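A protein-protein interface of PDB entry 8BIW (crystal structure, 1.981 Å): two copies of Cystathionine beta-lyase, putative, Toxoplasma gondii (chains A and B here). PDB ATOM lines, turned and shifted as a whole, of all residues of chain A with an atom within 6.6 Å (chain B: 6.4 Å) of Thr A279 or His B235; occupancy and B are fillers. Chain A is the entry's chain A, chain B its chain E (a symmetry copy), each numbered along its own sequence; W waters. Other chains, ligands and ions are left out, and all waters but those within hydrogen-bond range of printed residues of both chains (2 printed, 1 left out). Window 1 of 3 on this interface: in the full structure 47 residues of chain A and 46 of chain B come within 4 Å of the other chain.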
ATOM      1  N   TYR A  39      24.478  15.186  35.632  1.00  0.00           N
ATOM      2  CA  TYR A  39      24.949  14.811  34.302  1.00  0.00           C
ATOM      3  C   TYR A  39      25.724  15.953  33.666  1.00  0.00           C
ATOM      4  O   TYR A  39      26.740  15.727  33.008  1.00  0.00           O
ATOM      5  CB  TYR A  39      23.814  14.394  33.384  1.00  0.00           C
ATOM      6  CG  TYR A  39      23.391  12.967  33.610  1.00  0.00           C
ATOM      7  CD1 TYR A  39      22.445  12.675  34.589  1.00  0.00           C
ATOM      8  CD2 TYR A  39      23.968  11.914  32.867  1.00  0.00           C
ATOM      9  CE1 TYR A  39      22.030  11.338  34.831  1.00  0.00           C
ATOM     10  CE2 TYR A  39      23.573  10.590  33.086  1.00  0.00           C
ATOM     11  CZ  TYR A  39      22.595  10.324  34.063  1.00  0.00           C
ATOM     12  OH  TYR A  39      22.188   9.035  34.233  1.00  0.00           O
ATOM     13  N   VAL A  40      25.253  17.185  33.821  1.00  0.00           N
ATOM     14  CA  VAL A  40      25.995  18.282  33.174  1.00  0.00           C
ATOM     15  C   VAL A  40      27.326  18.567  33.878  1.00  0.00           C
ATOM     16  O   VAL A  40      28.367  18.755  33.226  1.00  0.00           O
ATOM     17  CB  VAL A  40      25.125  19.541  33.091  1.00  0.00           C
ATOM     18  CG1 VAL A  40      25.972  20.698  32.500  1.00  0.00           C
ATOM     19  CG2 VAL A  40      23.920  19.239  32.252  1.00  0.00           C
ATOM     20  N   ILE A  53      36.022  26.289  31.327  1.00  0.00           N
ATOM     21  CA  ILE A  53      34.790  25.705  31.825  1.00  0.00           C
ATOM     22  C   ILE A  53      34.776  24.197  31.623  1.00  0.00           C
ATOM     23  O   ILE A  53      34.149  23.474  32.408  1.00  0.00           O
ATOM     24  CB  ILE A  53      33.587  26.403  31.154  1.00  0.00           C
ATOM     25  CG1 ILE A  53      32.275  26.095  31.888  1.00  0.00           C
ATOM     26  CG2 ILE A  53      33.492  26.011  29.702  1.00  0.00           C
ATOM     27  CD1 ILE A  53      31.141  27.134  31.462  1.00  0.00           C
ATOM     28  N   LEU A  54      35.462  23.685  30.590  1.00  0.00           N
ATOM     29  CA  LEU A  54      35.699  22.240  30.405  1.00  0.00           C
ATOM     30  C   LEU A  54      37.088  21.882  30.944  1.00  0.00           C
ATOM     31  O   LEU A  54      38.017  22.654  30.795  1.00  0.00           O
ATOM     32  CB  LEU A  54      35.629  21.859  28.928  1.00  0.00           C
ATOM     33  CG  LEU A  54      34.347  22.332  28.208  1.00  0.00           C
ATOM     34  CD1 LEU A  54      34.318  21.816  26.786  1.00  0.00           C
ATOM     35  CD2 LEU A  54      33.051  21.864  28.988  1.00  0.00           C
ATOM     36  N   ASP A 233      28.337   7.321  25.536  1.00  0.00           N
ATOM     37  CA  ASP A 233      28.779   8.023  24.336  1.00  0.00           C
ATOM     38  C   ASP A 233      27.574   8.400  23.492  1.00  0.00           C
ATOM     39  O   ASP A 233      27.313   9.578  23.249  1.00  0.00           O
ATOM     40  CB  ASP A 233      29.731   7.115  23.546  1.00  0.00           C
ATOM     41  CG  ASP A 233      30.266   7.777  22.222  1.00  0.00           C
ATOM     42  OD1 ASP A 233      29.507   8.092  21.291  1.00  0.00           O
ATOM     43  OD2 ASP A 233      31.488   7.916  22.093  1.00  0.00           O
ATOM     44  N   HIS A 235      26.973   8.432  20.435  1.00  0.00           N
ATOM     45  CA  HIS A 235      27.209   9.094  19.169  1.00  0.00           C
ATOM     46  C   HIS A 235      28.018   8.251  18.198  1.00  0.00           C
ATOM     47  O   HIS A 235      28.473   8.792  17.197  1.00  0.00           O
ATOM     48  CB  HIS A 235      27.954  10.422  19.395  1.00  0.00           C
ATOM     49  CG  HIS A 235      27.115  11.485  20.029  1.00  0.00           C
ATOM     50  ND1 HIS A 235      26.812  11.494  21.377  1.00  0.00           N
ATOM     51  CD2 HIS A 235      26.536  12.592  19.505  1.00  0.00           C
ATOM     52  CE1 HIS A 235      26.084  12.569  21.656  1.00  0.00           C
ATOM     53  NE2 HIS A 235      25.922  13.261  20.538  1.00  0.00           N
ATOM     54  N   LEU A 274      32.989  12.740  28.625  1.00  0.00           N
ATOM     55  CA  LEU A 274      32.549  13.815  29.517  1.00  0.00           C
ATOM     56  C   LEU A 274      31.571  14.764  28.812  1.00  0.00           C
ATOM     57  O   LEU A 274      30.624  15.243  29.430  1.00  0.00           O
ATOM     58  CB  LEU A 274      33.762  14.598  30.029  1.00  0.00           C
ATOM     59  CG  LEU A 274      34.597  14.001  31.126  1.00  0.00           C
ATOM     60  CD1 LEU A 274      36.097  14.605  31.074  1.00  0.00           C
ATOM     61  CD2 LEU A 274      33.906  14.266  32.467  1.00  0.00           C
ATOM     62  N   LEU A 275      31.805  15.048  27.532  1.00  0.00           N
ATOM     63  CA  LEU A 275      30.880  15.877  26.761  1.00  0.00           C
ATOM     64  C   LEU A 275      29.549  15.148  26.493  1.00  0.00           C
ATOM     65  O   LEU A 275      28.474  15.703  26.738  1.00  0.00           O
ATOM     66  CB  LEU A 275      31.501  16.272  25.439  1.00  0.00           C
ATOM     67  CG  LEU A 275      32.542  17.387  25.215  1.00  0.00           C
ATOM     68  CD1 LEU A 275      32.870  17.521  23.737  1.00  0.00           C
ATOM     69  CD2 LEU A 275      32.115  18.730  25.775  1.00  0.00           C
ATOM     70  N   THR A 276      29.608  13.929  25.945  1.00  0.00           N
ATOM     71  CA  THR A 276      28.364  13.260  25.522  1.00  0.00           C
ATOM     72  C   THR A 276      27.501  12.892  26.725  1.00  0.00           C
ATOM     73  O   THR A 276      26.266  12.867  26.609  1.00  0.00           O
ATOM     74  CB  THR A 276      28.656  11.999  24.673  1.00  0.00           C
ATOM     75  OG1 THR A 276      29.468  11.097  25.415  1.00  0.00           O
ATOM     76  CG2 THR A 276      29.415  12.323  23.428  1.00  0.00           C
ATOM     77  N   LEU A 277      28.112  12.668  27.911  1.00  0.00           N
ATOM     78  CA  LEU A 277      27.292  12.293  29.063  1.00  0.00           C
ATOM     79  C   LEU A 277      26.341  13.411  29.470  1.00  0.00           C
ATOM     80  O   LEU A 277      25.326  13.144  30.115  1.00  0.00           O
ATOM     81  CB  LEU A 277      28.143  11.931  30.277  1.00  0.00           C
ATOM     82  CG  LEU A 277      28.380  10.452  30.527  1.00  0.00           C
ATOM     83  CD1 LEU A 277      29.353  10.312  31.730  1.00  0.00           C
ATOM     84  CD2 LEU A 277      26.994   9.688  30.760  1.00  0.00           C
ATOM     85  N   LYS A 278      26.693  14.662  29.178  1.00  0.00           N
ATOM     86  CA  LYS A 278      25.835  15.785  29.567  1.00  0.00           C
ATOM     87  C   LYS A 278      24.431  15.664  28.981  1.00  0.00           C
ATOM     88  O   LYS A 278      23.460  16.132  29.595  1.00  0.00           O
ATOM     89  CB  LYS A 278      26.481  17.105  29.124  1.00  0.00           C
ATOM     90  CG  LYS A 278      27.878  17.373  29.791  1.00  0.00           C
ATOM     91  CD  LYS A 278      28.511  18.641  29.160  1.00  0.00           C
ATOM     92  CE  LYS A 278      29.900  18.835  29.750  1.00  0.00           C
ATOM     93  NZ  LYS A 278      29.829  19.667  31.004  1.00  0.00           N
ATOM     94  N   THR A 279      24.282  15.062  27.800  1.00  0.00           N
ATOM     95  CA  THR A 279      22.965  14.983  27.180  1.00  0.00           C
ATOM     96  C   THR A 279      22.336  13.602  27.344  1.00  0.00           C
ATOM     97  O   THR A 279      21.322  13.334  26.703  1.00  0.00           O
ATOM     98  CB  THR A 279      23.035  15.324  25.680  1.00  0.00           C
ATOM     99  OG1 THR A 279      23.887  14.380  25.000  1.00  0.00           O
ATOM    100  CG2 THR A 279      23.527  16.806  25.404  1.00  0.00           C
ATOM    101  N   LEU A 280      22.914  12.704  28.158  1.00  0.00           N
ATOM    102  CA  LEU A 280      22.331  11.361  28.228  1.00  0.00           C
ATOM    103  C   LEU A 280      20.847  11.408  28.642  1.00  0.00           C
ATOM    104  O   LEU A 280      20.029  10.743  27.984  1.00  0.00           O
ATOM    105  CB  LEU A 280      23.141  10.449  29.163  1.00  0.00           C
ATOM    106  CG  LEU A 280      22.656   8.974  29.144  1.00  0.00           C
ATOM    107  CD1 LEU A 280      23.789   8.032  29.418  1.00  0.00           C
ATOM    108  CD2 LEU A 280      21.607   8.813  30.303  1.00  0.00           C
ATOM    109  N   PRO A 281      20.426  12.138  29.688  1.00  0.00           N
ATOM    110  CA  PRO A 281      18.969  12.163  29.994  1.00  0.00           C
ATOM    111  C   PRO A 281      18.084  12.585  28.816  1.00  0.00           C
ATOM    112  O   PRO A 281      17.108  11.881  28.500  1.00  0.00           O
ATOM    113  CB  PRO A 281      18.871  13.147  31.188  1.00  0.00           C
ATOM    114  CG  PRO A 281      20.282  12.970  31.902  1.00  0.00           C
ATOM    115  CD  PRO A 281      21.246  12.728  30.781  1.00  0.00           C
ATOM    116  N   ILE A 282      18.407  13.681  28.127  1.00  0.00           N
ATOM    117  CA  ILE A 282      17.497  14.066  27.043  1.00  0.00           C
ATOM    118  C   ILE A 282      17.593  13.119  25.859  1.00  0.00           C
ATOM    119  O   ILE A 282      16.594  12.911  25.144  1.00  0.00           O
ATOM    120  CB  ILE A 282      17.724  15.536  26.609  1.00  0.00           C
ATOM    121  CG1 ILE A 282      19.184  15.779  26.207  1.00  0.00           C
ATOM    122  CG2 ILE A 282      17.302  16.501  27.789  1.00  0.00           C
ATOM    123  CD1 ILE A 282      19.454  17.258  25.632  1.00  0.00           C
ATOM    124  N   ARG A 283      18.786  12.564  25.572  1.00  0.00           N
ATOM    125  CA  ARG A 283      18.863  11.582  24.494  1.00  0.00           C
ATOM    126  C   ARG A 283      18.000  10.361  24.809  1.00  0.00           C
ATOM    127  O   ARG A 283      17.258   9.879  23.955  1.00  0.00           O
ATOM    128  CB  ARG A 283      20.315  11.110  24.257  1.00  0.00           C
ATOM    129  CG  ARG A 283      21.216  12.148  23.502  1.00  0.00           C
ATOM    130  CD  ARG A 283      22.650  11.594  23.232  1.00  0.00           C
ATOM    131  NE  ARG A 283      23.562  11.617  24.409  1.00  0.00           N
ATOM    132  CZ  ARG A 283      23.992  10.507  25.023  1.00  0.00           C
ATOM    133  NH1 ARG A 283      23.580   9.310  24.596  1.00  0.00           N
ATOM    134  NH2 ARG A 283      24.860  10.576  26.032  1.00  0.00           N
ATOM    135  N   VAL A 284      18.210   9.767  25.977  1.00  0.00           N
ATOM    136  CA  VAL A 284      17.516   8.527  26.313  1.00  0.00           C
ATOM    137  C   VAL A 284      16.009   8.762  26.392  1.00  0.00           C
ATOM    138  O   VAL A 284      15.222   7.885  26.012  1.00  0.00           O
ATOM    139  CB  VAL A 284      18.086   7.962  27.645  1.00  0.00           C
ATOM    140  CG1 VAL A 284      17.191   6.815  28.165  1.00  0.00           C
ATOM    141  CG2 VAL A 284      19.557   7.420  27.422  1.00  0.00           C
ATOM    142  N   THR B 229      29.811  28.265  17.326  1.00  0.00           N
ATOM    143  CA  THR B 229      30.287  28.229  18.718  1.00  0.00           C
ATOM    144  C   THR B 229      29.149  28.035  19.714  1.00  0.00           C
ATOM    145  O   THR B 229      29.333  27.419  20.775  1.00  0.00           O
ATOM    146  CB  THR B 229      30.990  29.561  19.056  1.00  0.00           C
ATOM    147  OG1 THR B 229      31.960  29.872  18.046  1.00  0.00           O
ATOM    148  CG2 THR B 229      31.619  29.569  20.442  1.00  0.00           C
ATOM    149  N   LYS B 230      28.015  28.686  19.468  1.00  0.00           N
ATOM    150  CA  LYS B 230      27.022  28.871  20.523  1.00  0.00           C
ATOM    151  C   LYS B 230      26.108  27.647  20.637  1.00  0.00           C
ATOM    152  O   LYS B 230      26.385  26.736  21.413  1.00  0.00           O
ATOM    153  CB  LYS B 230      26.196  30.148  20.241  1.00  0.00           C
ATOM    154  CG  LYS B 230      27.027  31.431  20.072  1.00  0.00           C
ATOM    155  CD  LYS B 230      28.129  31.488  21.021  1.00  0.00           C
ATOM    156  CE  LYS B 230      28.692  32.943  21.268  1.00  0.00           C
ATOM    157  NZ  LYS B 230      28.621  33.939  20.171  1.00  0.00           N
ATOM    158  N   TYR B 231      25.040  27.584  19.849  1.00  0.00           N
ATOM    159  CA  TYR B 231      24.127  26.439  19.967  1.00  0.00           C
ATOM    160  C   TYR B 231      24.459  25.256  19.086  1.00  0.00           C
ATOM    161  O   TYR B 231      24.120  24.117  19.444  1.00  0.00           O
ATOM    162  CB  TYR B 231      22.713  26.860  19.600  1.00  0.00           C
ATOM    163  CG  TYR B 231      22.043  27.674  20.672  1.00  0.00           C
ATOM    164  CD1 TYR B 231      21.403  27.038  21.755  1.00  0.00           C
ATOM    165  CD2 TYR B 231      22.005  29.057  20.591  1.00  0.00           C
ATOM    166  CE1 TYR B 231      20.775  27.791  22.793  1.00  0.00           C
ATOM    167  CE2 TYR B 231      21.361  29.830  21.626  1.00  0.00           C
ATOM    168  CZ  TYR B 231      20.753  29.186  22.702  1.00  0.00           C
ATOM    169  OH  TYR B 231      20.135  29.933  23.675  1.00  0.00           O
ATOM    170  N   TYR B 232      24.974  25.490  17.867  1.00  0.00           N
ATOM    171  CA  TYR B 232      25.297  24.341  17.019  1.00  0.00           C
ATOM    172  C   TYR B 232      26.246  23.431  17.753  1.00  0.00           C
ATOM    173  O   TYR B 232      26.094  22.201  17.713  1.00  0.00           O
ATOM    174  CB  TYR B 232      25.975  24.744  15.688  1.00  0.00           C
ATOM    175  CG  TYR B 232      25.117  25.222  14.528  1.00  0.00           C
ATOM    176  CD1 TYR B 232      23.941  25.985  14.716  1.00  0.00           C
ATOM    177  CD2 TYR B 232      25.552  25.022  13.244  1.00  0.00           C
ATOM    178  CE1 TYR B 232      23.226  26.503  13.570  1.00  0.00           C
ATOM    179  CE2 TYR B 232      24.836  25.513  12.131  1.00  0.00           C
ATOM    180  CZ  TYR B 232      23.690  26.244  12.306  1.00  0.00           C
ATOM    181  OH  TYR B 232      23.044  26.671  11.156  1.00  0.00           O
ATOM    182  N   ASP B 233      27.258  24.028  18.399  1.00  0.00           N
ATOM    183  CA  ASP B 233      28.164  23.278  19.281  1.00  0.00           C
ATOM    184  C   ASP B 233      27.447  22.941  20.592  1.00  0.00           C
ATOM    185  O   ASP B 233      27.251  21.770  20.931  1.00  0.00           O
ATOM    186  CB  ASP B 233      29.442  24.098  19.511  1.00  0.00           C
ATOM    187  CG  ASP B 233      30.473  23.415  20.477  1.00  0.00           C
ATOM    188  OD1 ASP B 233      30.112  22.958  21.569  1.00  0.00           O
ATOM    189  OD2 ASP B 233      31.674  23.362  20.140  1.00  0.00           O
ATOM    190  N   GLY B 234      26.981  23.954  21.314  1.00  0.00           N
ATOM    191  CA  GLY B 234      26.199  23.690  22.502  1.00  0.00           C
ATOM    192  C   GLY B 234      26.949  23.065  23.654  1.00  0.00           C
ATOM    193  O   GLY B 234      26.326  22.751  24.681  1.00  0.00           O
ATOM    194  N   HIS B 235      28.269  22.885  23.547  1.00  0.00           N
ATOM    195  CA  HIS B 235      28.996  22.229  24.626  1.00  0.00           C
ATOM    196  C   HIS B 235      30.206  23.002  25.119  1.00  0.00           C
ATOM    197  O   HIS B 235      31.029  22.429  25.834  1.00  0.00           O
ATOM    198  CB  HIS B 235      29.457  20.854  24.161  1.00  0.00           C
ATOM    199  CG  HIS B 235      28.359  19.852  24.039  1.00  0.00           C
ATOM    200  ND1 HIS B 235      27.452  19.863  23.000  1.00  0.00           N
ATOM    201  CD2 HIS B 235      28.045  18.773  24.807  1.00  0.00           C
ATOM    202  CE1 HIS B 235      26.646  18.815  23.108  1.00  0.00           C
ATOM    203  NE2 HIS B 235      26.978  18.149  24.203  1.00  0.00           N
ATOM    204  N   ASN B 236      30.357  24.262  24.723  1.00  0.00           N
ATOM    205  CA  ASN B 236      31.517  25.086  25.060  1.00  0.00           C
ATOM    206  C   ASN B 236      32.813  24.447  24.587  1.00  0.00           C
ATOM    207  O   ASN B 236      33.862  24.683  25.183  1.00  0.00           O
ATOM    208  CB  ASN B 236      31.617  25.362  26.574  1.00  0.00           C
ATOM    209  CG  ASN B 236      30.586  26.369  27.060  1.00  0.00           C
ATOM    210  OD1 ASN B 236      30.460  27.441  26.502  1.00  0.00           O
ATOM    211  ND2 ASN B 236      29.827  26.010  28.116  1.00  0.00           N
ATOM    212  N   CYS B 237      32.727  23.599  23.567  1.00  0.00           N
ATOM    213  CA  CYS B 237      33.862  22.826  23.080  1.00  0.00           C
ATOM    214  C   CYS B 237      34.655  23.545  21.974  1.00  0.00           C
ATOM    215  O   CYS B 237      35.866  23.711  22.087  1.00  0.00           O
ATOM    216  CB  CYS B 237      33.343  21.482  22.565  1.00  0.00           C
ATOM    217  SG  CYS B 237      34.690  20.446  22.118  1.00  0.00           S
ATOM    218  N   THR B 238      33.996  24.022  20.925  1.00  0.00           N
ATOM    219  CA  THR B 238      34.699  24.550  19.755  1.00  0.00           C
ATOM    220  C   THR B 238      34.226  25.949  19.430  1.00  0.00           C
ATOM    221  O   THR B 238      33.099  26.316  19.745  1.00  0.00           O
ATOM    222  CB  THR B 238      34.434  23.738  18.471  1.00  0.00           C
ATOM    223  OG1 THR B 238      33.078  23.989  18.061  1.00  0.00           O
ATOM    224  CG2 THR B 238      34.601  22.297  18.697  1.00  0.00           C
ATOM    225  N   THR B 276      27.787  17.329  17.621  1.00  0.00           N
ATOM    226  CA  THR B 276      26.892  18.044  18.543  1.00  0.00           C
ATOM    227  C   THR B 276      25.622  18.537  17.840  1.00  0.00           C
ATOM    228  O   THR B 276      24.583  18.715  18.499  1.00  0.00           O
ATOM    229  CB  THR B 276      27.622  19.257  19.167  1.00  0.00           C
ATOM    230  OG1 THR B 276      28.056  20.117  18.117  1.00  0.00           O
ATOM    231  CG2 THR B 276      28.830  18.862  19.953  1.00  0.00           C
ATOM    232  N   THR B 279      22.103  16.635  18.352  1.00  0.00           N
ATOM    233  CA  THR B 279      21.240  16.828  19.494  1.00  0.00           C
ATOM    234  C   THR B 279      20.702  18.251  19.582  1.00  0.00           C
ATOM    235  O   THR B 279      20.079  18.590  20.576  1.00  0.00           O
ATOM    236  CB  THR B 279      21.960  16.446  20.792  1.00  0.00           C
ATOM    237  OG1 THR B 279      23.108  17.287  20.968  1.00  0.00           O
ATOM    238  CG2 THR B 279      22.387  14.946  20.790  1.00  0.00           C
ATOM    239  N   ILE B 282      16.854  18.385  20.633  1.00  0.00           N
ATOM    240  CA  ILE B 282      16.495  18.047  22.017  1.00  0.00           C
ATOM    241  C   ILE B 282      17.173  18.976  23.027  1.00  0.00           C
ATOM    242  O   ILE B 282      16.610  19.242  24.103  1.00  0.00           O
ATOM    243  CB  ILE B 282      16.771  16.561  22.367  1.00  0.00           C
ATOM    244  CG1 ILE B 282      18.239  16.202  22.120  1.00  0.00           C
ATOM    245  CG2 ILE B 282      15.832  15.634  21.546  1.00  0.00           C
ATOM    246  CD1 ILE B 282      18.579  14.652  22.450  1.00  0.00           C
ATOM    247  N   ARG B 283      18.382  19.476  22.743  1.00  0.00           N
ATOM    248  CA  ARG B 283      18.976  20.448  23.656  1.00  0.00           C
ATOM    249  C   ARG B 283      18.135  21.724  23.723  1.00  0.00           C
ATOM    250  O   ARG B 283      17.918  22.280  24.802  1.00  0.00           O
ATOM    251  CB  ARG B 283      20.401  20.797  23.211  1.00  0.00           C
ATOM    252  CG  ARG B 283      21.417  19.700  23.568  1.00  0.00           C
ATOM    253  CD  ARG B 283      22.838  20.148  23.165  1.00  0.00           C
ATOM    254  NE  ARG B 283      23.130  20.059  21.703  1.00  0.00           N
ATOM    255  CZ  ARG B 283      23.368  21.139  20.954  1.00  0.00           C
ATOM    256  NH1 ARG B 283      23.244  22.336  21.501  1.00  0.00           N
ATOM    257  NH2 ARG B 283      23.715  21.052  19.678  1.00  0.00           N
ATOM    258  N   GLY B 362      24.497  29.547  24.843  1.00  0.00           N
ATOM    259  CA  GLY B 362      23.986  28.481  23.992  1.00  0.00           C
ATOM    260  C   GLY B 362      24.305  27.071  24.464  1.00  0.00           C
ATOM    261  O   GLY B 362      23.939  26.097  23.773  1.00  0.00           O
ATOM    262  N   ALA B 363      25.002  26.935  25.582  1.00  0.00           N
ATOM    263  CA  ALA B 363      25.688  25.711  25.983  1.00  0.00           C
ATOM    264  C   ALA B 363      24.804  24.905  26.919  1.00  0.00           C
ATOM    265  O   ALA B 363      23.867  25.441  27.514  1.00  0.00           O
ATOM    266  CB  ALA B 363      26.998  26.057  26.706  1.00  0.00           C
ATOM    267  N   CYS B 364      25.149  23.602  27.069  1.00  0.00           N
ATOM    268  CA  CYS B 364      24.525  22.739  28.080  1.00  0.00           C
ATOM    269  C   CYS B 364      24.687  23.302  29.484  1.00  0.00           C
ATOM    270  O   CYS B 364      23.857  23.029  30.370  1.00  0.00           O
ATOM    271  CB  CYS B 364      25.168  21.337  28.039  1.00  0.00           C
ATOM    272  SG  CYS B 364      24.773  20.396  26.551  1.00  0.00           S
ATOM    273  N   GLU B 365      25.821  23.965  29.735  1.00  0.00           N
ATOM    274  CA  GLU B 365      26.136  24.656  30.995  1.00  0.00           C
ATOM    275  C   GLU B 365      25.483  26.050  31.007  1.00  0.00           C
ATOM    276  O   GLU B 365      25.784  26.856  30.135  1.00  0.00           O
ATOM    277  CB  GLU B 365      27.645  24.851  31.118  1.00  0.00           C
ATOM    278  CG  GLU B 365      28.455  23.564  31.221  1.00  0.00           C
ATOM    279  CD  GLU B 365      28.763  22.903  29.847  1.00  0.00           C
ATOM    280  OE1 GLU B 365      28.572  23.487  28.744  1.00  0.00           O
ATOM    281  OE2 GLU B 365      29.232  21.763  29.887  1.00  0.00           O
ATOM    282  N   ILE B 400      20.941  22.886  30.292  1.00  0.00           N
ATOM    283  CA  ILE B 400      20.027  21.735  30.419  1.00  0.00           C
ATOM    284  C   ILE B 400      20.090  21.106  31.814  1.00  0.00           C
ATOM    285  O   ILE B 400      19.703  19.934  32.003  1.00  0.00           O
ATOM    286  CB  ILE B 400      20.275  20.689  29.317  1.00  0.00           C
ATOM    287  CG1 ILE B 400      21.670  20.040  29.452  1.00  0.00           C
ATOM    288  CG2 ILE B 400      20.117  21.347  27.900  1.00  0.00           C
ATOM    289  CD1 ILE B 400      21.899  18.962  28.335  1.00  0.00           C
HETATM  290  O   HOH W   1      25.343  15.974  22.344  1.00  0.00           O
HETATM  291  O   HOH W   2      28.432  14.831  19.870  1.00  0.00           O
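The backbone carbonyl oxygen (O) of Val A40 is in hydrogen-bond range of the side-chain amino group (NZ) of Lys A278 (2.8 Å).
The guanidinium group of Arg A283 sits at hydrogen-bond distance from the backbone carbonyl oxygen of Thr A276 (2.7 Å).
O of Tyr B231 sits at hydrogen-bond distance from NH1 of Arg B283, at 2.9 Å.
The backbone carbonyl oxygen (O) of Tyr B232 sits at hydrogen-bond distance from the guanidinium group (NH2) of Arg B283 (3.3 Å).
The backbone NH (N) of Cys B364 sits at hydrogen-bond distance from the backbone carbonyl oxygen (O) of Gly B234 (2.8 Å).
The backbone NH (N) of Ile B400 lies within hydrogen-bond range of the backbone carbonyl oxygen (O) of Cys B364, 2.9 Å away.
Cys B364 touches Val A40 (O to CG1, 3.8 Å).
Val A40 touches Ile B400 (CG2 to CG1, 3.7 Å).
CG2 of Ile A53 touches CB of Asn B236, at 3.7 Å.
His B235 touches Leu A54.
SG of Cys B237 touches CD1 of Leu A275, at 3.8 Å.
Ile B400 touches Lys A278.
Thr A279 touches His B235 (CG2 to NE2, 3.9 Å).
Ile B400 touches Thr A279.
Ile A282 touches Ile B282.
Ile A282 touches Arg B283.
NZ of Lys A278 is in salt-bridge range of OE2 of Glu B365 (2.4 Å).
Water W1 lies within hydrogen-bond range of OG1 of Thr B279 (2.9 Å), NE2 of His B235 (3.3 Å), NE2 of His A235 (3.3 Å) and OG1 of Thr A279 (3.4 Å).
Water W2 bridges NE2 of His A235 (3.0 Å) and N of Thr B276 (3.4 Å).
His A235 touches Thr B279, and with the chains exchanged Thr A279 touches His B235.
Ile B282 touches its own counterpart, Ile A282.
Ile A282 touches Arg B283, and with the chains exchanged Arg A283 touches Ile B282.
6 positions are printed for both chains.
Of the 18 pairs that touch across the chains among the printed residues, 5 have their exchanged pair printed and touching as well.
Printed residues of chain B within 4 Å of Leu A275: His B235 (3.7 Å) and Cys B237 (3.8 Å).
Val A284 touches none of the printed residues of chain B.
His B235 touches just these residues of chain A: Leu A54 (3.5 Å), Leu A275 (3.7 Å) and Thr A279 (3.9 Å).
Printed residues of chain A within 4 Å of Glu B365: Leu A54 and Lys A278.
The nearest printed residue of chain B that does not touch Thr A279 is Arg B283 (4.02 Å).
The nearest residue of chain A that does not touch His B235 is Lys A278 (4.4 Å).
The nearest printed residue of chain A that does not touch Thr B279 is Arg A283 (4.1 Å).
Hydrophobic or aromatic side chains of chain B within 4 Å of the printed part of chain A: His B235, Ile B282 and Ile B400.
Printed residues of chain A that touch a printed residue of chain B: Val A40, Ile A53, Leu A54, His A235, Leu A275, Lys A278, Thr A279, Ile A282 and Arg A283.
Hydrophobic or aromatic side chains of chain A that line the printed part of chain B: Val A40, Ile A53, Leu A54, His A235, Leu A275 and Ile A282.
Among the printed residues, 18 pairs touch across the chains.
Among the printed residues, Asp or Glu carboxylates within 4 Å of a Lys or Arg side-chain nitrogen of the other chain: Lys A278 with Glu B365 (2.4 Å).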
